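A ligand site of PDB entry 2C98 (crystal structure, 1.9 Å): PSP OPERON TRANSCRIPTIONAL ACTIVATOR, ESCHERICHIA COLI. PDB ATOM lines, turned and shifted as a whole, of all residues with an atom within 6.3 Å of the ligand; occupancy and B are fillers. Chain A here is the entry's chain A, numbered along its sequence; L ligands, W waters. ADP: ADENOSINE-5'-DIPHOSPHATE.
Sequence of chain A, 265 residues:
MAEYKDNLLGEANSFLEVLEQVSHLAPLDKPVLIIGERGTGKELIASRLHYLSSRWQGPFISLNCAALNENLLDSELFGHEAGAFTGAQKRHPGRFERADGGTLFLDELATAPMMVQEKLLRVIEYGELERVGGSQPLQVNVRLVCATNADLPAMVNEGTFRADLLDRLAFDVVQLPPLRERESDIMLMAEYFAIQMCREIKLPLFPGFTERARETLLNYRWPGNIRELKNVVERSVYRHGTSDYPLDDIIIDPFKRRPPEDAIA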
ATOM      1  N   LEU A   8      23.102  13.894  -4.513  1.00  0.00           N
ATOM      2  CA  LEU A   8      23.234  12.447  -4.901  1.00  0.00           C
ATOM      3  C   LEU A   8      23.348  12.423  -6.403  1.00  0.00           C
ATOM      4  O   LEU A   8      22.742  13.247  -7.099  1.00  0.00           O
ATOM      5  CB  LEU A   8      22.008  11.631  -4.504  1.00  0.00           C
ATOM      6  CG  LEU A   8      21.610  11.478  -3.041  1.00  0.00           C
ATOM      7  CD1 LEU A   8      20.423  10.577  -2.893  1.00  0.00           C
ATOM      8  CD2 LEU A   8      22.773  10.945  -2.220  1.00  0.00           C
ATOM      9  N   LEU A   9      24.092  11.465  -6.930  1.00  0.00           N
ATOM     10  CA  LEU A   9      24.314  11.389  -8.367  1.00  0.00           C
ATOM     11  C   LEU A   9      23.342  10.428  -8.986  1.00  0.00           C
ATOM     12  O   LEU A   9      22.984   9.412  -8.380  1.00  0.00           O
ATOM     13  CB  LEU A   9      25.743  10.936  -8.649  1.00  0.00           C
ATOM     14  CG  LEU A   9      26.861  11.775  -8.015  1.00  0.00           C
ATOM     15  CD1 LEU A   9      28.228  11.149  -8.140  1.00  0.00           C
ATOM     16  CD2 LEU A   9      26.838  13.207  -8.579  1.00  0.00           C
ATOM     17  N   GLY A  10      22.915  10.732 -10.188  1.00  0.00           N
ATOM     18  CA  GLY A  10      22.146   9.795 -10.993  1.00  0.00           C
ATOM     19  C   GLY A  10      20.989  10.480 -11.688  1.00  0.00           C
ATOM     20  O   GLY A  10      20.410  11.391 -11.152  1.00  0.00           O
ATOM     21  N   PHE A  15      16.327   5.134 -10.593  1.00  0.00           N
ATOM     22  CA  PHE A  15      16.854   5.823  -9.406  1.00  0.00           C
ATOM     23  C   PHE A  15      15.984   7.037  -9.041  1.00  0.00           C
ATOM     24  O   PHE A  15      15.663   7.258  -7.888  1.00  0.00           O
ATOM     25  CB  PHE A  15      18.263   6.301  -9.670  1.00  0.00           C
ATOM     26  CG  PHE A  15      18.881   7.024  -8.492  1.00  0.00           C
ATOM     27  CD1 PHE A  15      19.149   6.309  -7.300  1.00  0.00           C
ATOM     28  CD2 PHE A  15      19.157   8.371  -8.552  1.00  0.00           C
ATOM     29  CE1 PHE A  15      19.690   6.965  -6.172  1.00  0.00           C
ATOM     30  CE2 PHE A  15      19.706   9.024  -7.440  1.00  0.00           C
ATOM     31  CZ  PHE A  15      19.978   8.331  -6.268  1.00  0.00           C
ATOM     32  N   GLU A  37      21.576  -4.545  -3.570  1.00  0.00           N
ATOM     33  CA  GLU A  37      22.901  -5.123  -3.467  1.00  0.00           C
ATOM     34  C   GLU A  37      23.816  -4.249  -2.602  1.00  0.00           C
ATOM     35  O   GLU A  37      23.555  -3.081  -2.372  1.00  0.00           O
ATOM     36  CB  GLU A  37      23.485  -5.308  -4.856  1.00  0.00           C
ATOM     37  CG  GLU A  37      22.832  -6.418  -5.686  1.00  0.00           C
ATOM     38  CD  GLU A  37      23.442  -6.632  -7.057  1.00  0.00           C
ATOM     39  OE1 GLU A  37      24.554  -6.137  -7.309  1.00  0.00           O
ATOM     40  OE2 GLU A  37      22.780  -7.313  -7.916  1.00  0.00           O
ATOM     41  N   ARG A  38      24.956  -4.797  -2.200  1.00  0.00           N
ATOM     42  CA  ARG A  38      25.929  -3.990  -1.479  1.00  0.00           C
ATOM     43  C   ARG A  38      26.397  -2.836  -2.357  1.00  0.00           C
ATOM     44  O   ARG A  38      26.544  -2.987  -3.553  1.00  0.00           O
ATOM     45  CB  ARG A  38      27.154  -4.827  -1.082  1.00  0.00           C
ATOM     46  CG  ARG A  38      28.008  -5.316  -2.219  1.00  0.00           C
ATOM     47  CD  ARG A  38      29.127  -6.247  -1.705  1.00  0.00           C
ATOM     48  NE  ARG A  38      30.216  -6.457  -2.668  1.00  0.00           N
ATOM     49  CZ  ARG A  38      30.298  -7.508  -3.437  1.00  0.00           C
ATOM     50  NH1 ARG A  38      29.374  -8.497  -3.421  1.00  0.00           N
ATOM     51  NH2 ARG A  38      31.313  -7.557  -4.264  1.00  0.00           N
ATOM     52  N   GLY A  39      26.599  -1.681  -1.723  1.00  0.00           N
ATOM     53  CA  GLY A  39      27.076  -0.501  -2.416  1.00  0.00           C
ATOM     54  C   GLY A  39      26.104   0.250  -3.286  1.00  0.00           C
ATOM     55  O   GLY A  39      26.547   1.073  -4.128  1.00  0.00           O
ATOM     56  N   THR A  40      24.810  -0.018  -3.163  1.00  0.00           N
ATOM     57  CA  THR A  40      23.809   0.659  -4.011  1.00  0.00           C
ATOM     58  C   THR A  40      23.175   1.851  -3.375  1.00  0.00           C
ATOM     59  O   THR A  40      22.344   2.547  -3.992  1.00  0.00           O
ATOM     60  CB  THR A  40      22.655  -0.294  -4.424  1.00  0.00           C
ATOM     61  OG1 THR A  40      22.090  -0.915  -3.255  1.00  0.00           O
ATOM     62  CG2 THR A  40      23.151  -1.425  -5.306  1.00  0.00           C
ATOM     63  N   GLY A  41      23.522   2.098  -2.132  1.00  0.00           N
ATOM     64  CA  GLY A  41      23.061   3.263  -1.380  1.00  0.00           C
ATOM     65  C   GLY A  41      21.980   2.956  -0.364  1.00  0.00           C
ATOM     66  O   GLY A  41      21.202   3.814  -0.057  1.00  0.00           O
ATOM     67  N   LYS A  42      21.986   1.758   0.216  1.00  0.00           N
ATOM     68  CA  LYS A  42      20.993   1.368   1.206  1.00  0.00           C
ATOM     69  C   LYS A  42      21.016   2.213   2.455  1.00  0.00           C
ATOM     70  O   LYS A  42      19.972   2.748   2.867  1.00  0.00           O
ATOM     71  CB  LYS A  42      21.134  -0.126   1.598  1.00  0.00           C
ATOM     72  CG  LYS A  42      20.974  -1.161   0.522  1.00  0.00           C
ATOM     73  CD  LYS A  42      21.482  -2.574   1.082  1.00  0.00           C
ATOM     74  CE  LYS A  42      22.975  -2.677   1.131  1.00  0.00           C
ATOM     75  NZ  LYS A  42      23.593  -3.931   1.968  1.00  0.00           N
ATOM     76  N   GLU A  43      22.188   2.376   3.032  1.00  0.00           N
ATOM     77  CA  GLU A  43      22.344   3.257   4.168  1.00  0.00           C
ATOM     78  C   GLU A  43      22.090   4.702   3.823  1.00  0.00           C
ATOM     79  O   GLU A  43      21.469   5.427   4.606  1.00  0.00           O
ATOM     80  CB  GLU A  43      23.690   3.099   4.851  1.00  0.00           C
ATOM     81  CG  GLU A  43      23.792   3.864   6.160  1.00  0.00           C
ATOM     82  CD  GLU A  43      24.855   3.330   7.105  1.00  0.00           C
ATOM     83  OE1 GLU A  43      25.038   3.917   8.207  1.00  0.00           O
ATOM     84  OE2 GLU A  43      25.480   2.303   6.789  1.00  0.00           O
ATOM     85  N   LEU A  44      22.517   5.140   2.621  1.00  0.00           N
ATOM     86  CA  LEU A  44      22.226   6.507   2.235  1.00  0.00           C
ATOM     87  C   LEU A  44      20.736   6.786   2.148  1.00  0.00           C
ATOM     88  O   LEU A  44      20.246   7.827   2.599  1.00  0.00           O
ATOM     89  CB  LEU A  44      22.898   6.752   0.921  1.00  0.00           C
ATOM     90  CG  LEU A  44      22.666   8.096   0.292  1.00  0.00           C
ATOM     91  CD1 LEU A  44      23.954   8.388  -0.534  1.00  0.00           C
ATOM     92  CD2 LEU A  44      21.469   8.050  -0.585  1.00  0.00           C
ATOM     93  N   ILE A  45      19.989   5.865   1.576  1.00  0.00           N
ATOM     94  CA  ILE A  45      18.532   5.966   1.487  1.00  0.00           C
ATOM     95  C   ILE A  45      17.891   5.888   2.846  1.00  0.00           C
ATOM     96  O   ILE A  45      16.929   6.643   3.078  1.00  0.00           O
ATOM     97  CB  ILE A  45      17.959   4.864   0.520  1.00  0.00           C
ATOM     98  CG1 ILE A  45      18.405   5.172  -0.909  1.00  0.00           C
ATOM     99  CG2 ILE A  45      16.434   4.792   0.618  1.00  0.00           C
ATOM    100  CD1 ILE A  45      17.824   6.408  -1.573  1.00  0.00           C
ATOM    101  N   PHE A 105      18.378   1.761  11.466  1.00  0.00           N
ATOM    102  CA  PHE A 105      18.620   1.091  10.193  1.00  0.00           C
ATOM    103  C   PHE A 105      19.297  -0.267  10.464  1.00  0.00           C
ATOM    104  O   PHE A 105      20.450  -0.311  10.931  1.00  0.00           O
ATOM    105  CB  PHE A 105      19.535   1.936   9.319  1.00  0.00           C
ATOM    106  CG  PHE A 105      19.983   1.275   8.073  1.00  0.00           C
ATOM    107  CD1 PHE A 105      19.076   0.685   7.223  1.00  0.00           C
ATOM    108  CD2 PHE A 105      21.314   1.210   7.736  1.00  0.00           C
ATOM    109  CE1 PHE A 105      19.508   0.057   6.037  1.00  0.00           C
ATOM    110  CE2 PHE A 105      21.734   0.556   6.592  1.00  0.00           C
ATOM    111  CZ  PHE A 105      20.824  -0.011   5.751  1.00  0.00           C
ATOM    112  N   ASP A 107      20.815  -3.322   8.672  1.00  0.00           N
ATOM    113  CA  ASP A 107      21.294  -3.867   7.419  1.00  0.00           C
ATOM    114  C   ASP A 107      21.512  -5.368   7.518  1.00  0.00           C
ATOM    115  O   ASP A 107      21.666  -5.925   8.607  1.00  0.00           O
ATOM    116  CB  ASP A 107      22.545  -3.116   7.032  1.00  0.00           C
ATOM    117  CG  ASP A 107      22.945  -3.302   5.585  1.00  0.00           C
ATOM    118  OD1 ASP A 107      22.173  -3.827   4.751  1.00  0.00           O
ATOM    119  OD2 ASP A 107      24.064  -2.940   5.186  1.00  0.00           O
ATOM    120  N   LEU A 176      16.305  -0.781  -4.785  1.00  0.00           N
ATOM    121  CA  LEU A 176      17.401  -0.009  -5.290  1.00  0.00           C
ATOM    122  C   LEU A 176      18.071  -0.755  -6.400  1.00  0.00           C
ATOM    123  O   LEU A 176      18.531  -1.905  -6.239  1.00  0.00           O
ATOM    124  CB  LEU A 176      18.464   0.258  -4.212  1.00  0.00           C
ATOM    125  CG  LEU A 176      18.351   1.376  -3.252  1.00  0.00           C
ATOM    126  CD1 LEU A 176      19.551   1.318  -2.279  1.00  0.00           C
ATOM    127  CD2 LEU A 176      18.406   2.683  -4.014  1.00  0.00           C
ATOM    128  N   ARG A 182      21.338   1.003 -14.116  1.00  0.00           N
ATOM    129  CA  ARG A 182      21.071   2.437 -13.948  1.00  0.00           C
ATOM    130  C   ARG A 182      21.453   3.256 -15.189  1.00  0.00           C
ATOM    131  O   ARG A 182      21.900   4.393 -15.089  1.00  0.00           O
ATOM    132  CB  ARG A 182      21.746   2.996 -12.696  1.00  0.00           C
ATOM    133  CG  ARG A 182      21.069   2.518 -11.403  1.00  0.00           C
ATOM    134  CD  ARG A 182      21.676   3.008 -10.117  1.00  0.00           C
ATOM    135  NE  ARG A 182      21.806   4.426 -10.172  1.00  0.00           N
ATOM    136  CZ  ARG A 182      22.076   5.201  -9.139  1.00  0.00           C
ATOM    137  NH1 ARG A 182      22.191   4.684  -7.858  1.00  0.00           N
ATOM    138  NH2 ARG A 182      22.179   6.502  -9.401  1.00  0.00           N
ATOM    139  N   MET A 189      28.782   8.983 -12.600  1.00  0.00           N
ATOM    140  CA  MET A 189      29.442   8.782 -11.356  1.00  0.00           C
ATOM    141  C   MET A 189      30.952   8.586 -11.554  1.00  0.00           C
ATOM    142  O   MET A 189      31.744   9.083 -10.745  1.00  0.00           O
ATOM    143  CB  MET A 189      28.848   7.531 -10.681  1.00  0.00           C
ATOM    144  CG  MET A 189      27.408   7.752 -10.220  1.00  0.00           C
ATOM    145  SD  MET A 189      26.961   6.320  -9.219  1.00  0.00           S
ATOM    146  CE  MET A 189      25.468   6.776  -8.616  1.00  0.00           C
ATOM    147  N   PHE A 193      33.764  10.837  -9.706  1.00  0.00           N
ATOM    148  CA  PHE A 193      34.785  10.234  -8.865  1.00  0.00           C
ATOM    149  C   PHE A 193      36.189  10.501  -9.370  1.00  0.00           C
ATOM    150  O   PHE A 193      37.103  10.766  -8.575  1.00  0.00           O
ATOM    151  CB  PHE A 193      34.581   8.720  -8.677  1.00  0.00           C
ATOM    152  CG  PHE A 193      33.326   8.367  -7.948  1.00  0.00           C
ATOM    153  CD1 PHE A 193      32.548   7.300  -8.358  1.00  0.00           C
ATOM    154  CD2 PHE A 193      32.926   9.103  -6.833  1.00  0.00           C
ATOM    155  CE1 PHE A 193      31.390   6.986  -7.703  1.00  0.00           C
ATOM    156  CE2 PHE A 193      31.754   8.778  -6.178  1.00  0.00           C
ATOM    157  CZ  PHE A 193      30.993   7.714  -6.624  1.00  0.00           C
ATOM    158  N   ILE A 226      28.482   1.060  -6.241  1.00  0.00           N
ATOM    159  CA  ILE A 226      29.049   2.391  -6.198  1.00  0.00           C
ATOM    160  C   ILE A 226      30.269   2.460  -5.351  1.00  0.00           C
ATOM    161  O   ILE A 226      31.195   3.184  -5.688  1.00  0.00           O
ATOM    162  CB  ILE A 226      27.967   3.444  -5.743  1.00  0.00           C
ATOM    163  CG1 ILE A 226      26.767   3.333  -6.672  1.00  0.00           C
ATOM    164  CG2 ILE A 226      28.580   4.844  -5.739  1.00  0.00           C
ATOM    165  CD1 ILE A 226      25.517   4.117  -6.200  1.00  0.00           C
ATOM    166  N   ARG A 227      30.353   1.636  -4.311  1.00  0.00           N
ATOM    167  CA  ARG A 227      31.549   1.564  -3.509  1.00  0.00           C
ATOM    168  C   ARG A 227      32.748   1.059  -4.350  1.00  0.00           C
ATOM    169  O   ARG A 227      33.875   1.624  -4.303  1.00  0.00           O
ATOM    170  CB  ARG A 227      31.273   0.657  -2.310  1.00  0.00           C
ATOM    171  CG  ARG A 227      32.320   0.737  -1.280  1.00  0.00           C
ATOM    172  CD  ARG A 227      32.033  -0.189  -0.131  1.00  0.00           C
ATOM    173  NE  ARG A 227      31.175   0.412   0.889  1.00  0.00           N
ATOM    174  CZ  ARG A 227      29.901   0.101   1.101  1.00  0.00           C
ATOM    175  NH1 ARG A 227      29.290  -0.785   0.359  1.00  0.00           N
ATOM    176  NH2 ARG A 227      29.238   0.713   2.064  1.00  0.00           N
ATOM    177  N   LYS A 230      33.792   3.734  -7.188  1.00  0.00           N
ATOM    178  CA  LYS A 230      34.662   4.775  -6.647  1.00  0.00           C
ATOM    179  C   LYS A 230      36.130   4.326  -6.521  1.00  0.00           C
ATOM    180  O   LYS A 230      37.050   5.044  -6.894  1.00  0.00           O
ATOM    181  CB  LYS A 230      34.144   5.287  -5.291  1.00  0.00           C
ATOM    182  CG  LYS A 230      34.943   6.494  -4.780  1.00  0.00           C
ATOM    183  CD  LYS A 230      34.255   7.076  -3.524  1.00  0.00           C
ATOM    184  CE  LYS A 230      34.988   8.266  -2.999  1.00  0.00           C
ATOM    185  NZ  LYS A 230      36.128   7.799  -2.088  1.00  0.00           N
HETATM  186  PB  ADP L   1      25.259   0.324   1.026  1.00  0.00           P
HETATM  187  O1B ADP L   1      26.423  -0.708   1.033  1.00  0.00           O
HETATM  188  O2B ADP L   1      24.532   0.447   2.330  1.00  0.00           O
HETATM  189  O3B ADP L   1      24.360   0.144  -0.096  1.00  0.00           O
HETATM  190  PA  ADP L   1      26.017   3.123   1.144  1.00  0.00           P
HETATM  191  O1A ADP L   1      26.881   3.218   2.274  1.00  0.00           O
HETATM  192  O2A ADP L   1      24.639   3.664   1.295  1.00  0.00           O
HETATM  193  O3A ADP L   1      26.149   1.595   0.860  1.00  0.00           O
HETATM  194  O5' ADP L   1      26.670   3.667  -0.243  1.00  0.00           O
HETATM  195  C5' ADP L   1      27.908   3.151  -0.649  1.00  0.00           C
HETATM  196  C4' ADP L   1      28.757   4.323  -1.105  1.00  0.00           C
HETATM  197  O4' ADP L   1      28.196   4.811  -2.287  1.00  0.00           O
HETATM  198  C3' ADP L   1      28.736   5.511  -0.147  1.00  0.00           C
HETATM  199  O3' ADP L   1      30.034   6.086  -0.175  1.00  0.00           O
HETATM  200  C2' ADP L   1      27.745   6.479  -0.730  1.00  0.00           C
HETATM  201  O2' ADP L   1      28.025   7.848  -0.555  1.00  0.00           O
HETATM  202  C1' ADP L   1      27.847   6.172  -2.190  1.00  0.00           C
HETATM  203  N9  ADP L   1      26.600   6.405  -2.925  1.00  0.00           N
HETATM  204  C8  ADP L   1      25.506   5.574  -2.949  1.00  0.00           C
HETATM  205  N7  ADP L   1      24.555   6.112  -3.757  1.00  0.00           N
HETATM  206  C5  ADP L   1      25.024   7.296  -4.264  1.00  0.00           C
HETATM  207  C6  ADP L   1      24.481   8.234  -5.134  1.00  0.00           C
HETATM  208  N6  ADP L   1      23.314   8.099  -5.740  1.00  0.00           N
HETATM  209  N1  ADP L   1      25.267   9.314  -5.465  1.00  0.00           N
HETATM  210  C2  ADP L   1      26.506   9.509  -4.929  1.00  0.00           C
HETATM  211  N3  ADP L   1      27.067   8.573  -4.083  1.00  0.00           N
HETATM  212  C4  ADP L   1      26.320   7.482  -3.756  1.00  0.00           C
HETATM  213  O   HOH W   1      29.626  10.116  -0.193  1.00  0.00           O
HETATM  214  O   HOH W   2      31.610   5.226  -2.865  1.00  0.00           O
HETATM  215  O   HOH W   3      27.683   2.757   4.946  1.00  0.00           O
HETATM  216  O   HOH W   4      30.834   6.081   2.711  1.00  0.00           O
HETATM  217  O   HOH W   5      22.370   5.257  -4.962  1.00  0.00           O
HETATM  218  O   HOH W   6      25.172  -0.365   4.567  1.00  0.00           O
HETATM  219  O   HOH W   7      29.663   9.651  -3.202  1.00  0.00           O
HETATM  220  O   HOH W   8      26.011   6.142   3.242  1.00  0.00           O
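Water W6 lies within hydrogen-bond range of an oxygen (O2B) of the ligand (2.5 Å), the side-chain carboxylate of Asp 107 (2.9 Å) and the side-chain carboxylate of Glu 43 (3.5 Å).
Water W5 lies within hydrogen-bond range of N7 of the ligand, O of Thr 40 and NH1 of Arg 182.
Water W3 bridges O1A of the ligand (2.8 Å) and OE2 of Glu 43 (2.9 Å).
A nitrogen (N1) of the ligand lies within hydrogen-bond range of the backbone NH of Leu 9, at 2.9 Å.
The backbone carbonyl oxygen (O) of Leu 9 lies within hydrogen-bond range of a nitrogen (N6) of the ligand.
O3B of the ligand sits at hydrogen-bond distance from N of Lys 42 (2.9 Å).
N of Leu 44 is in hydrogen-bond range of O2A of the ligand (2.9 Å).
The backbone NH (N) of Gly 39 is in hydrogen-bond range of an oxygen (O1B) of the ligand (2.9 Å).
An oxygen (O3B) of the ligand is in hydrogen-bond range of the backbone NH of Gly 41, at 2.9 Å.
An oxygen (O1B) of the ligand lies within salt-bridge range of the guanidinium group (NH1) of Arg 227, 2.9 Å away.
An oxygen (O3B) of the ligand lies within hydrogen-bond range of the backbone NH (N) of Thr 40 (3.1 Å).
N of Glu 43 lies within hydrogen-bond range of O2B of the ligand (3.1 Å).
Residues that only touch the ligand: Ile 226, Phe 15, Leu 8 and Met 189.
Hydrophobic or aromatic side chains within 4 Å of the ligand: Leu 8, Leu 9, Phe 15, Leu 44, Met 189 and Ile 226.
Within 4 Å of the ligand: Leu 8, Leu 9, Phe 15, Gly 39, Thr 40, Gly 41, Lys 42, Glu 43, Leu 44, Met 189, Ile 226 and Arg 227.
The backbone carbonyl oxygen (O) of Leu 9 is in hydrogen-bond range of the guanidinium group (NH2) of Arg 182.
NZ of Lys 42 lies within salt-bridge range of OD1 of Asp 107 (3.1 Å).
N of Ile 226 sits at hydrogen-bond distance from O of Gly 39, at 2.9 Å.
The side-chain hydroxyl (OG1) of Thr 40 lies within hydrogen-bond range of the backbone carbonyl oxygen (O) of Glu 37, at 2.8 Å.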
